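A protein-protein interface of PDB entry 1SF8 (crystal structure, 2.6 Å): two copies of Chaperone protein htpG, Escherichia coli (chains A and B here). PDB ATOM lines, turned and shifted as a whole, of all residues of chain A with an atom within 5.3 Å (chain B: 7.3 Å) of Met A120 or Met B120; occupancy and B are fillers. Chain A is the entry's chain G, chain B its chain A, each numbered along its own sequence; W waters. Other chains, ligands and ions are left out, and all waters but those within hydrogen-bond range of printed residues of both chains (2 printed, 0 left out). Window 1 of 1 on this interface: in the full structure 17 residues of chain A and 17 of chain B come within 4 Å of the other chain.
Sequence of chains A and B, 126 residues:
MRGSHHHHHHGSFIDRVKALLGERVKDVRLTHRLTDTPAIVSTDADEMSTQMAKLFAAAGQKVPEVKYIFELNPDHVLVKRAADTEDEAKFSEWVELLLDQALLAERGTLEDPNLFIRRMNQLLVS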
ATOM      1  N   LEU A  97      -5.169 -21.552  10.964  1.00  0.00           N
ATOM      2  CA  LEU A  97      -5.082 -20.309  11.731  1.00  0.00           C
ATOM      3  C   LEU A  97      -4.117 -20.475  12.905  1.00  0.00           C
ATOM      4  O   LEU A  97      -3.244 -19.637  13.128  1.00  0.00           O
ATOM      5  CB  LEU A  97      -6.456 -19.903  12.272  1.00  0.00           C
ATOM      6  CG  LEU A  97      -6.385 -18.666  13.173  1.00  0.00           C
ATOM      7  CD1 LEU A  97      -6.318 -17.424  12.277  1.00  0.00           C
ATOM      8  CD2 LEU A  97      -7.586 -18.599  14.140  1.00  0.00           C
ATOM      9  N   GLN A 101      -0.463 -18.965  13.795  1.00  0.00           N
ATOM     10  CA  GLN A 101      -0.239 -18.192  15.020  1.00  0.00           C
ATOM     11  C   GLN A 101       1.044 -18.650  15.711  1.00  0.00           C
ATOM     12  O   GLN A 101       1.819 -17.847  16.224  1.00  0.00           O
ATOM     13  CB  GLN A 101      -1.407 -18.347  15.994  1.00  0.00           C
ATOM     14  CG  GLN A 101      -2.690 -17.721  15.502  1.00  0.00           C
ATOM     15  CD  GLN A 101      -3.793 -17.695  16.557  1.00  0.00           C
ATOM     16  OE1 GLN A 101      -4.798 -16.989  16.408  1.00  0.00           O
ATOM     17  NE2 GLN A 101      -3.612 -18.469  17.618  1.00  0.00           N
ATOM     18  N   PHE A 116      -2.880 -15.011   6.186  1.00  0.00           N
ATOM     19  CA  PHE A 116      -3.182 -15.173   7.609  1.00  0.00           C
ATOM     20  C   PHE A 116      -4.211 -14.128   8.017  1.00  0.00           C
ATOM     21  O   PHE A 116      -5.211 -14.425   8.677  1.00  0.00           O
ATOM     22  CB  PHE A 116      -1.890 -14.992   8.424  1.00  0.00           C
ATOM     23  CG  PHE A 116      -2.088 -14.965   9.920  1.00  0.00           C
ATOM     24  CD1 PHE A 116      -2.518 -16.087  10.610  1.00  0.00           C
ATOM     25  CD2 PHE A 116      -1.797 -13.818  10.643  1.00  0.00           C
ATOM     26  CE1 PHE A 116      -2.656 -16.064  12.020  1.00  0.00           C
ATOM     27  CE2 PHE A 116      -1.928 -13.777  12.050  1.00  0.00           C
ATOM     28  CZ  PHE A 116      -2.358 -14.905  12.738  1.00  0.00           C
ATOM     29  N   ILE A 117      -3.964 -12.892   7.605  1.00  0.00           N
ATOM     30  CA  ILE A 117      -4.858 -11.807   7.935  1.00  0.00           C
ATOM     31  C   ILE A 117      -6.254 -12.069   7.363  1.00  0.00           C
ATOM     32  O   ILE A 117      -7.256 -11.810   8.030  1.00  0.00           O
ATOM     33  CB  ILE A 117      -4.276 -10.471   7.434  1.00  0.00           C
ATOM     34  CG1 ILE A 117      -2.937 -10.225   8.144  1.00  0.00           C
ATOM     35  CG2 ILE A 117      -5.253  -9.325   7.701  1.00  0.00           C
ATOM     36  CD1 ILE A 117      -2.202  -8.969   7.715  1.00  0.00           C
ATOM     37  N   ARG A 118      -6.346 -12.610   6.154  1.00  0.00           N
ATOM     38  CA  ARG A 118      -7.671 -12.847   5.604  1.00  0.00           C
ATOM     39  C   ARG A 118      -8.417 -13.890   6.432  1.00  0.00           C
ATOM     40  O   ARG A 118      -9.606 -13.745   6.744  1.00  0.00           O
ATOM     41  CB  ARG A 118      -7.591 -13.290   4.155  1.00  0.00           C
ATOM     42  CG  ARG A 118      -8.774 -12.761   3.359  1.00  0.00           C
ATOM     43  CD  ARG A 118      -9.146 -13.649   2.186  1.00  0.00           C
ATOM     44  NE  ARG A 118      -7.994 -14.314   1.571  1.00  0.00           N
ATOM     45  CZ  ARG A 118      -6.958 -13.687   1.011  1.00  0.00           C
ATOM     46  NH1 ARG A 118      -6.913 -12.353   0.979  1.00  0.00           N
ATOM     47  NH2 ARG A 118      -5.967 -14.398   0.473  1.00  0.00           N
ATOM     48  N   ARG A 119      -7.696 -14.944   6.779  1.00  0.00           N
ATOM     49  CA  ARG A 119      -8.213 -16.018   7.609  1.00  0.00           C
ATOM     50  C   ARG A 119      -8.798 -15.511   8.942  1.00  0.00           C
ATOM     51  O   ARG A 119      -9.980 -15.720   9.226  1.00  0.00           O
ATOM     52  CB  ARG A 119      -7.076 -16.970   7.900  1.00  0.00           C
ATOM     53  CG  ARG A 119      -7.484 -18.274   8.495  1.00  0.00           C
ATOM     54  CD  ARG A 119      -7.303 -19.301   7.442  1.00  0.00           C
ATOM     55  NE  ARG A 119      -6.014 -19.173   6.778  1.00  0.00           N
ATOM     56  CZ  ARG A 119      -5.397 -20.212   6.239  1.00  0.00           C
ATOM     57  NH1 ARG A 119      -5.983 -21.376   6.328  1.00  0.00           N
ATOM     58  NH2 ARG A 119      -4.232 -20.117   5.614  1.00  0.00           N
ATOM     59  N   MET A 120      -7.996 -14.846   9.767  1.00  0.00           N
ATOM     60  CA  MET A 120      -8.563 -14.423  11.032  1.00  0.00           C
ATOM     61  C   MET A 120      -9.777 -13.552  10.830  1.00  0.00           C
ATOM     62  O   MET A 120     -10.741 -13.645  11.593  1.00  0.00           O
ATOM     63  CB  MET A 120      -7.521 -13.737  11.944  1.00  0.00           C
ATOM     64  CG  MET A 120      -6.899 -12.513  11.329  1.00  0.00           C
ATOM     65  SD  MET A 120      -5.836 -11.455  12.547  1.00  0.00           S
ATOM     66  CE  MET A 120      -7.450 -10.616  13.549  1.00  0.00           C
ATOM     67  N   ASN A 121      -9.747 -12.733   9.786  1.00  0.00           N
ATOM     68  CA  ASN A 121     -10.862 -11.830   9.505  1.00  0.00           C
ATOM     69  C   ASN A 121     -12.158 -12.549   9.229  1.00  0.00           C
ATOM     70  O   ASN A 121     -13.238 -12.147   9.697  1.00  0.00           O
ATOM     71  CB  ASN A 121     -10.515 -10.918   8.350  1.00  0.00           C
ATOM     72  CG  ASN A 121      -9.638  -9.786   8.799  1.00  0.00           C
ATOM     73  OD1 ASN A 121      -9.519  -9.552  10.010  1.00  0.00           O
ATOM     74  ND2 ASN A 121      -9.025  -9.071   7.858  1.00  0.00           N
ATOM     75  N   GLN A 122     -12.046 -13.634   8.477  1.00  0.00           N
ATOM     76  CA  GLN A 122     -13.210 -14.435   8.162  1.00  0.00           C
ATOM     77  C   GLN A 122     -13.687 -15.113   9.421  1.00  0.00           C
ATOM     78  O   GLN A 122     -14.877 -15.080   9.750  1.00  0.00           O
ATOM     79  CB  GLN A 122     -12.856 -15.484   7.129  1.00  0.00           C
ATOM     80  CG  GLN A 122     -12.695 -14.892   5.776  1.00  0.00           C
ATOM     81  CD  GLN A 122     -12.325 -15.920   4.752  1.00  0.00           C
ATOM     82  OE1 GLN A 122     -12.251 -17.114   5.045  1.00  0.00           O
ATOM     83  NE2 GLN A 122     -12.093 -15.467   3.532  1.00  0.00           N
ATOM     84  N   LEU A 123     -12.755 -15.737  10.123  1.00  0.00           N
ATOM     85  CA  LEU A 123     -13.111 -16.427  11.335  1.00  0.00           C
ATOM     86  C   LEU A 123     -13.671 -15.471  12.380  1.00  0.00           C
ATOM     87  O   LEU A 123     -14.511 -15.857  13.177  1.00  0.00           O
ATOM     88  CB  LEU A 123     -11.900 -17.189  11.855  1.00  0.00           C
ATOM     89  CG  LEU A 123     -11.596 -18.396  10.961  1.00  0.00           C
ATOM     90  CD1 LEU A 123     -10.271 -19.029  11.338  1.00  0.00           C
ATOM     91  CD2 LEU A 123     -12.718 -19.407  11.095  1.00  0.00           C
ATOM     92  N   LEU A 124     -13.238 -14.216  12.365  1.00  0.00           N
ATOM     93  CA  LEU A 124     -13.748 -13.272  13.341  1.00  0.00           C
ATOM     94  C   LEU A 124     -15.192 -12.928  13.047  1.00  0.00           C
ATOM     95  O   LEU A 124     -15.938 -12.486  13.926  1.00  0.00           O
ATOM     96  CB  LEU A 124     -12.904 -11.996  13.345  1.00  0.00           C
ATOM     97  CG  LEU A 124     -11.554 -12.093  14.060  1.00  0.00           C
ATOM     98  CD1 LEU A 124     -10.778 -10.862  13.713  1.00  0.00           C
ATOM     99  CD2 LEU A 124     -11.722 -12.226  15.582  1.00  0.00           C
ATOM    100  N   VAL A 125     -15.573 -13.136  11.791  1.00  0.00           N
ATOM    101  CA  VAL A 125     -16.917 -12.841  11.305  1.00  0.00           C
ATOM    102  C   VAL A 125     -17.824 -14.075  11.328  1.00  0.00           C
ATOM    103  O   VAL A 125     -19.044 -13.955  11.225  1.00  0.00           O
ATOM    104  CB  VAL A 125     -16.825 -12.249   9.887  1.00  0.00           C
ATOM    105  CG1 VAL A 125     -18.102 -12.490   9.108  1.00  0.00           C
ATOM    106  CG2 VAL A 125     -16.545 -10.766  10.000  1.00  0.00           C
ATOM    107  N   LEU B  78     -15.787  -5.773   9.257  1.00  0.00           N
ATOM    108  CA  LEU B  78     -15.080  -5.536  10.520  1.00  0.00           C
ATOM    109  C   LEU B  78     -14.937  -4.069  10.898  1.00  0.00           C
ATOM    110  O   LEU B  78     -14.979  -3.734  12.077  1.00  0.00           O
ATOM    111  CB  LEU B  78     -13.700  -6.197  10.492  1.00  0.00           C
ATOM    112  CG  LEU B  78     -13.786  -7.723  10.517  1.00  0.00           C
ATOM    113  CD1 LEU B  78     -12.393  -8.320  10.572  1.00  0.00           C
ATOM    114  CD2 LEU B  78     -14.614  -8.159  11.714  1.00  0.00           C
ATOM    115  N   GLU B  93     -10.263  -2.833  21.374  1.00  0.00           N
ATOM    116  CA  GLU B  93      -9.724  -4.100  20.904  1.00  0.00           C
ATOM    117  C   GLU B  93      -9.732  -4.152  19.378  1.00  0.00           C
ATOM    118  O   GLU B  93      -8.767  -4.631  18.766  1.00  0.00           O
ATOM    119  CB  GLU B  93     -10.537  -5.275  21.440  1.00  0.00           C
ATOM    120  CG  GLU B  93     -10.603  -5.368  22.944  1.00  0.00           C
ATOM    121  CD  GLU B  93     -11.265  -6.656  23.405  1.00  0.00           C
ATOM    122  OE1 GLU B  93     -10.598  -7.723  23.381  1.00  0.00           O
ATOM    123  OE2 GLU B  93     -12.464  -6.604  23.776  1.00  0.00           O
ATOM    124  N   TRP B  94     -10.816  -3.661  18.769  1.00  0.00           N
ATOM    125  CA  TRP B  94     -10.929  -3.661  17.311  1.00  0.00           C
ATOM    126  C   TRP B  94      -9.891  -2.741  16.655  1.00  0.00           C
ATOM    127  O   TRP B  94      -9.110  -3.187  15.806  1.00  0.00           O
ATOM    128  CB  TRP B  94     -12.346  -3.250  16.859  1.00  0.00           C
ATOM    129  CG  TRP B  94     -13.396  -4.309  17.078  1.00  0.00           C
ATOM    130  CD1 TRP B  94     -14.478  -4.229  17.908  1.00  0.00           C
ATOM    131  CD2 TRP B  94     -13.399  -5.643  16.544  1.00  0.00           C
ATOM    132  NE1 TRP B  94     -15.146  -5.438  17.938  1.00  0.00           N
ATOM    133  CE2 TRP B  94     -14.502  -6.320  17.111  1.00  0.00           C
ATOM    134  CE3 TRP B  94     -12.572  -6.334  15.650  1.00  0.00           C
ATOM    135  CZ2 TRP B  94     -14.798  -7.651  16.815  1.00  0.00           C
ATOM    136  CZ3 TRP B  94     -12.868  -7.662  15.353  1.00  0.00           C
ATOM    137  CH2 TRP B  94     -13.973  -8.306  15.939  1.00  0.00           C
ATOM    138  N   LEU B  97      -6.633  -4.245  16.998  1.00  0.00           N
ATOM    139  CA  LEU B  97      -6.490  -5.416  16.149  1.00  0.00           C
ATOM    140  C   LEU B  97      -6.300  -5.052  14.677  1.00  0.00           C
ATOM    141  O   LEU B  97      -5.541  -5.708  13.951  1.00  0.00           O
ATOM    142  CB  LEU B  97      -7.705  -6.326  16.285  1.00  0.00           C
ATOM    143  CG  LEU B  97      -7.501  -7.526  15.361  1.00  0.00           C
ATOM    144  CD1 LEU B  97      -6.496  -8.457  16.017  1.00  0.00           C
ATOM    145  CD2 LEU B  97      -8.822  -8.229  15.081  1.00  0.00           C
ATOM    146  N   LEU B  98      -6.998  -4.007  14.239  1.00  0.00           N
ATOM    147  CA  LEU B  98      -6.917  -3.552  12.854  1.00  0.00           C
ATOM    148  C   LEU B  98      -5.592  -2.863  12.578  1.00  0.00           C
ATOM    149  O   LEU B  98      -4.998  -3.041  11.512  1.00  0.00           O
ATOM    150  CB  LEU B  98      -8.078  -2.605  12.548  1.00  0.00           C
ATOM    151  CG  LEU B  98      -9.435  -3.322  12.530  1.00  0.00           C
ATOM    152  CD1 LEU B  98     -10.570  -2.333  12.443  1.00  0.00           C
ATOM    153  CD2 LEU B  98      -9.448  -4.292  11.366  1.00  0.00           C
ATOM    154  N   GLN B 101      -2.829  -5.385  12.324  1.00  0.00           N
ATOM    155  CA  GLN B 101      -3.068  -6.128  11.110  1.00  0.00           C
ATOM    156  C   GLN B 101      -2.443  -5.360   9.947  1.00  0.00           C
ATOM    157  O   GLN B 101      -1.674  -5.913   9.158  1.00  0.00           O
ATOM    158  CB  GLN B 101      -4.564  -6.238  10.965  1.00  0.00           C
ATOM    159  CG  GLN B 101      -5.061  -7.385  10.161  1.00  0.00           C
ATOM    160  CD  GLN B 101      -6.568  -7.308  10.036  1.00  0.00           C
ATOM    161  OE1 GLN B 101      -7.111  -6.271   9.644  1.00  0.00           O
ATOM    162  NE2 GLN B 101      -7.252  -8.394  10.366  1.00  0.00           N
ATOM    163  N   LEU B 104       1.275  -5.401  10.381  1.00  0.00           N
ATOM    164  CA  LEU B 104       1.882  -6.669  10.013  1.00  0.00           C
ATOM    165  C   LEU B 104       1.990  -6.808   8.502  1.00  0.00           C
ATOM    166  O   LEU B 104       2.931  -7.419   7.994  1.00  0.00           O
ATOM    167  CB  LEU B 104       1.078  -7.830  10.578  1.00  0.00           C
ATOM    168  CG  LEU B 104       1.449  -9.244  10.136  1.00  0.00           C
ATOM    169  CD1 LEU B 104       2.937  -9.554  10.340  1.00  0.00           C
ATOM    170  CD2 LEU B 104       0.590 -10.182  10.956  1.00  0.00           C
ATOM    171  N   LEU B 110       5.924  -7.494  13.744  1.00  0.00           N
ATOM    172  CA  LEU B 110       5.233  -6.736  14.762  1.00  0.00           C
ATOM    173  C   LEU B 110       6.133  -6.550  15.968  1.00  0.00           C
ATOM    174  O   LEU B 110       7.027  -7.359  16.229  1.00  0.00           O
ATOM    175  CB  LEU B 110       3.952  -7.444  15.182  1.00  0.00           C
ATOM    176  CG  LEU B 110       2.735  -7.191  14.295  1.00  0.00           C
ATOM    177  CD1 LEU B 110       1.643  -8.164  14.677  1.00  0.00           C
ATOM    178  CD2 LEU B 110       2.265  -5.750  14.440  1.00  0.00           C
ATOM    179  N   PRO B 113       4.255  -9.558  18.676  1.00  0.00           N
ATOM    180  CA  PRO B 113       3.542 -10.618  17.951  1.00  0.00           C
ATOM    181  C   PRO B 113       2.536 -11.312  18.843  1.00  0.00           C
ATOM    182  O   PRO B 113       1.384 -11.523  18.469  1.00  0.00           O
ATOM    183  CB  PRO B 113       4.657 -11.570  17.545  1.00  0.00           C
ATOM    184  CG  PRO B 113       5.798 -10.670  17.333  1.00  0.00           C
ATOM    185  CD  PRO B 113       5.707  -9.713  18.510  1.00  0.00           C
ATOM    186  N   ASN B 114       2.987 -11.677  20.032  1.00  0.00           N
ATOM    187  CA  ASN B 114       2.133 -12.364  20.980  1.00  0.00           C
ATOM    188  C   ASN B 114       0.976 -11.544  21.463  1.00  0.00           C
ATOM    189  O   ASN B 114      -0.059 -12.085  21.808  1.00  0.00           O
ATOM    190  CB  ASN B 114       2.955 -12.813  22.172  1.00  0.00           C
ATOM    191  CG  ASN B 114       3.867 -13.942  21.827  1.00  0.00           C
ATOM    192  OD1 ASN B 114       3.487 -15.106  21.920  1.00  0.00           O
ATOM    193  ND2 ASN B 114       5.077 -13.614  21.397  1.00  0.00           N
ATOM    194  N   LEU B 115       1.141 -10.236  21.524  1.00  0.00           N
ATOM    195  CA  LEU B 115       0.036  -9.429  21.995  1.00  0.00           C
ATOM    196  C   LEU B 115      -1.064  -9.485  20.937  1.00  0.00           C
ATOM    197  O   LEU B 115      -2.248  -9.537  21.251  1.00  0.00           O
ATOM    198  CB  LEU B 115       0.499  -7.999  22.210  1.00  0.00           C
ATOM    199  CG  LEU B 115      -0.640  -7.032  22.471  1.00  0.00           C
ATOM    200  CD1 LEU B 115      -1.421  -7.446  23.722  1.00  0.00           C
ATOM    201  CD2 LEU B 115      -0.066  -5.647  22.605  1.00  0.00           C
ATOM    202  N   PHE B 116      -0.640  -9.480  19.678  1.00  0.00           N
ATOM    203  CA  PHE B 116      -1.535  -9.535  18.529  1.00  0.00           C
ATOM    204  C   PHE B 116      -2.323 -10.841  18.573  1.00  0.00           C
ATOM    205  O   PHE B 116      -3.550 -10.858  18.498  1.00  0.00           O
ATOM    206  CB  PHE B 116      -0.693  -9.474  17.255  1.00  0.00           C
ATOM    207  CG  PHE B 116      -1.488  -9.450  15.998  1.00  0.00           C
ATOM    208  CD1 PHE B 116      -2.559  -8.588  15.862  1.00  0.00           C
ATOM    209  CD2 PHE B 116      -1.162 -10.282  14.939  1.00  0.00           C
ATOM    210  CE1 PHE B 116      -3.294  -8.550  14.688  1.00  0.00           C
ATOM    211  CE2 PHE B 116      -1.898 -10.245  13.753  1.00  0.00           C
ATOM    212  CZ  PHE B 116      -2.964  -9.377  13.637  1.00  0.00           C
ATOM    213  N   ILE B 117      -1.596 -11.935  18.711  1.00  0.00           N
ATOM    214  CA  ILE B 117      -2.200 -13.244  18.765  1.00  0.00           C
ATOM    215  C   ILE B 117      -3.144 -13.369  19.931  1.00  0.00           C
ATOM    216  O   ILE B 117      -4.183 -14.032  19.858  1.00  0.00           O
ATOM    217  CB  ILE B 117      -1.122 -14.283  18.899  1.00  0.00           C
ATOM    218  CG1 ILE B 117      -0.237 -14.200  17.656  1.00  0.00           C
ATOM    219  CG2 ILE B 117      -1.742 -15.660  19.177  1.00  0.00           C
ATOM    220  CD1 ILE B 117       0.811 -15.246  17.598  1.00  0.00           C
ATOM    221  N   ARG B 118      -2.789 -12.709  21.015  1.00  0.00           N
ATOM    222  CA  ARG B 118      -3.595 -12.771  22.215  1.00  0.00           C
ATOM    223  C   ARG B 118      -4.913 -12.049  22.006  1.00  0.00           C
ATOM    224  O   ARG B 118      -5.967 -12.607  22.280  1.00  0.00           O
ATOM    225  CB  ARG B 118      -2.822 -12.141  23.374  1.00  0.00           C
ATOM    226  CG  ARG B 118      -2.923 -12.882  24.704  1.00  0.00           C
ATOM    227  CD  ARG B 118      -2.102 -12.163  25.775  1.00  0.00           C
ATOM    228  NE  ARG B 118      -0.693 -12.162  25.404  1.00  0.00           N
ATOM    229  CZ  ARG B 118       0.118 -11.123  25.544  1.00  0.00           C
ATOM    230  NH1 ARG B 118      -0.331  -9.980  26.056  1.00  0.00           N
ATOM    231  NH2 ARG B 118       1.379 -11.231  25.146  1.00  0.00           N
ATOM    232  N   ARG B 119      -4.859 -10.821  21.497  1.00  0.00           N
ATOM    233  CA  ARG B 119      -6.081 -10.050  21.297  1.00  0.00           C
ATOM    234  C   ARG B 119      -6.979 -10.643  20.199  1.00  0.00           C
ATOM    235  O   ARG B 119      -8.199 -10.503  20.211  1.00  0.00           O
ATOM    236  CB  ARG B 119      -5.723  -8.581  21.004  1.00  0.00           C
ATOM    237  CG  ARG B 119      -4.711  -8.456  19.905  1.00  0.00           C
ATOM    238  CD  ARG B 119      -4.318  -6.997  19.540  1.00  0.00           C
ATOM    239  NE  ARG B 119      -3.554  -6.191  20.509  1.00  0.00           N
ATOM    240  CZ  ARG B 119      -4.117  -5.387  21.405  1.00  0.00           C
ATOM    241  NH1 ARG B 119      -5.433  -5.320  21.465  1.00  0.00           N
ATOM    242  NH2 ARG B 119      -3.390  -4.565  22.156  1.00  0.00           N
ATOM    243  N   MET B 120      -6.346 -11.322  19.258  1.00  0.00           N
ATOM    244  CA  MET B 120      -7.032 -11.964  18.151  1.00  0.00           C
ATOM    245  C   MET B 120      -7.930 -13.034  18.774  1.00  0.00           C
ATOM    246  O   MET B 120      -9.162 -12.986  18.668  1.00  0.00           O
ATOM    247  CB  MET B 120      -5.990 -12.619  17.260  1.00  0.00           C
ATOM    248  CG  MET B 120      -6.463 -13.041  15.908  1.00  0.00           C
ATOM    249  SD  MET B 120      -5.001 -14.051  15.172  1.00  0.00           S
ATOM    250  CE  MET B 120      -3.720 -12.501  15.258  1.00  0.00           C
ATOM    251  N   ASN B 121      -7.284 -13.998  19.433  1.00  0.00           N
ATOM    252  CA  ASN B 121      -7.984 -15.098  20.073  1.00  0.00           C
ATOM    253  C   ASN B 121      -9.022 -14.616  21.082  1.00  0.00           C
ATOM    254  O   ASN B 121     -10.023 -15.287  21.306  1.00  0.00           O
ATOM    255  CB  ASN B 121      -7.010 -16.046  20.776  1.00  0.00           C
ATOM    256  CG  ASN B 121      -6.033 -16.716  19.827  1.00  0.00           C
ATOM    257  OD1 ASN B 121      -6.351 -17.016  18.670  1.00  0.00           O
ATOM    258  ND2 ASN B 121      -4.838 -16.995  20.331  1.00  0.00           N
ATOM    259  N   GLN B 122      -8.798 -13.471  21.711  1.00  0.00           N
ATOM    260  CA  GLN B 122      -9.785 -12.997  22.675  1.00  0.00           C
ATOM    261  C   GLN B 122     -11.096 -12.629  21.955  1.00  0.00           C
ATOM    262  O   GLN B 122     -12.182 -12.923  22.441  1.00  0.00           O
ATOM    263  CB  GLN B 122      -9.241 -11.798  23.461  1.00  0.00           C
ATOM    264  CG  GLN B 122     -10.204 -11.261  24.518  1.00  0.00           C
ATOM    265  CD  GLN B 122     -10.698 -12.358  25.473  1.00  0.00           C
ATOM    266  OE1 GLN B 122      -9.893 -13.024  26.147  1.00  0.00           O
ATOM    267  NE2 GLN B 122     -12.028 -12.543  25.540  1.00  0.00           N
ATOM    268  N   LEU B 123     -10.990 -11.995  20.791  1.00  0.00           N
ATOM    269  CA  LEU B 123     -12.170 -11.624  20.029  1.00  0.00           C
ATOM    270  C   LEU B 123     -12.741 -12.871  19.356  1.00  0.00           C
ATOM    271  O   LEU B 123     -13.900 -12.885  18.975  1.00  0.00           O
ATOM    272  CB  LEU B 123     -11.809 -10.568  18.979  1.00  0.00           C
ATOM    273  CG  LEU B 123     -11.478  -9.186  19.554  1.00  0.00           C
ATOM    274  CD1 LEU B 123     -10.692  -8.347  18.556  1.00  0.00           C
ATOM    275  CD2 LEU B 123     -12.786  -8.484  19.942  1.00  0.00           C
ATOM    276  N   LEU B 124     -11.933 -13.920  19.217  1.00  0.00           N
ATOM    277  CA  LEU B 124     -12.409 -15.144  18.584  1.00  0.00           C
ATOM    278  C   LEU B 124     -13.230 -16.030  19.494  1.00  0.00           C
ATOM    279  O   LEU B 124     -14.012 -16.861  19.039  1.00  0.00           O
ATOM    280  CB  LEU B 124     -11.245 -15.967  18.059  1.00  0.00           C
ATOM    281  CG  LEU B 124     -10.694 -15.517  16.720  1.00  0.00           C
ATOM    282  CD1 LEU B 124      -9.404 -16.255  16.456  1.00  0.00           C
ATOM    283  CD2 LEU B 124     -11.709 -15.790  15.618  1.00  0.00           C
ATOM    284  N   VAL B 125     -13.051 -15.863  20.790  1.00  0.00           N
ATOM    285  CA  VAL B 125     -13.765 -16.688  21.741  1.00  0.00           C
ATOM    286  C   VAL B 125     -14.956 -15.969  22.335  1.00  0.00           C
ATOM    287  O   VAL B 125     -15.923 -16.600  22.746  1.00  0.00           O
ATOM    288  CB  VAL B 125     -12.832 -17.135  22.863  1.00  0.00           C
ATOM    289  CG1 VAL B 125     -13.619 -17.856  23.919  1.00  0.00           C
ATOM    290  CG2 VAL B 125     -11.761 -18.052  22.301  1.00  0.00           C
ATOM    291  N   SER B 126     -14.896 -14.646  22.370  1.00  0.00           N
ATOM    292  CA  SER B 126     -15.997 -13.877  22.931  1.00  0.00           C
ATOM    293  C   SER B 126     -17.211 -13.837  21.997  1.00  0.00           C
ATOM    294  O   SER B 126     -17.333 -14.745  21.135  1.00  0.00           O
ATOM    295  CB  SER B 126     -15.531 -12.457  23.262  1.00  0.00           C
ATOM    296  OG  SER B 126     -14.912 -11.850  22.144  1.00  0.00           O
ATOM    297  OXT SER B 126     -18.036 -12.905  22.153  1.00  0.00           O
HETATM  298  O   HOH W   1     -15.799 -16.066  16.338  1.00  0.00           O
HETATM  299  O   HOH W   2     -16.230 -13.646  16.666  1.00  0.00           O
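Leu A97 touches Leu B124, and with the chains exchanged Leu A124 touches Leu B97. Gln A101 touches Met B120, and with the chains exchanged Met A120 touches Gln B101. Leu A123 touches Leu B124, and with the chains exchanged Leu A124 touches Leu B123. Leu B124 touches its own counterpart, Leu A124. 12 positions are printed for both chains.
The side-chain sulfur (SD) of Met B120 sits close to the side-chain amide oxygen (OE1) of Gln A101 (3.2 Å). The side-chain amide oxygen (OD1) of Asn A121 sits at hydrogen-bond distance from the side-chain amide nitrogen (NE2) of Gln B101, 2.6 Å away. The side-chain amide oxygen (OE1) of Gln A101 sits close to the side-chain amide oxygen (OD1) of Asn B121 (2.7 Å). The side-chain sulfur (SD) of Met B120 lies close to the side-chain sulfur (SD) of Met A120.
Water W2 bridges the backbone carbonyl oxygen (O) of Leu A124 and the backbone carbonyl oxygen (O) of Leu B123. Water W1 bridges the backbone carbonyl oxygen (O) of Leu B124 and the backbone carbonyl oxygen (O) of Leu A123.
Among the printed residues, pairs that only touch across the chains: Leu A97 with Leu B124 (3.8 Å), Gln A101 with Ile B117 (3.1 Å), Phe A116 with Phe B116 (3.9 Å), Phe A116 with Met B120 (3.7 Å), Ile A117 with Gln B101 (3.1 Å), Met A120 with Leu B97 (3.2 Å), Met A120 with Gln B101 (3.9 Å), Met A120 with Phe B116 (3.7 Å), Asn A121 with Leu B78 (3.2 Å), Leu A123 with Leu B124 (3.7 Å), Leu A124 with Leu B97 (3.6 Å), Leu A124 with Leu B123 (3.8 Å), Leu A124 with Leu B124 (3.6 Å) and Val A125 with Leu B78 (3.7 Å).
Of chain A, only Gln A101, Phe A116 and Met A120 come within 4 Å of Met B120. Printed residues of chain B within 4 Å of Leu A124: Leu B97 (3.6 Å), Leu B123 (3.8 Å) and Leu B124 (3.6 Å). Printed residues of chain B within 4 Å of Leu A123: Leu B124 (3.7 Å). Printed residues of chain A within 4 Å of Leu B97: Met A120 and Leu A124. The nearest residue of chain A that does not touch Met B120 is Leu A124 (4.1 Å). The nearest printed residue of chain B that does not touch Ile A117 is Leu B104 (4.4 Å).
The backbone carbonyl oxygen of Ile A117 lies close to the side-chain amide nitrogen of Asn A121. OG of Ser B126 sits close to O of Leu B123. O of Ile B117 is in hydrogen-bond range of ND2 of Asn B121, at 3.1 Å.
Of the 12 printed residues of chain A, 9 touch a printed residue of chain B. Printed residues of chain A that touch a printed residue of chain B: Leu A97, Gln A101, Phe A116, Ile A117, Met A120, Asn A121, Leu A123, Leu A124 and Val A125. Hydrophobic or aromatic side chains of chain A within 4 Å of the printed part of chain B: Leu A97, Phe A116, Ile A117, Met A120, Leu A124 and Val A125. Along chain A the printed residues that touch a printed residue of chain B span positions 97 to 125. Of the 22 printed residues of chain B, 9 touch a printed residue of chain A.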
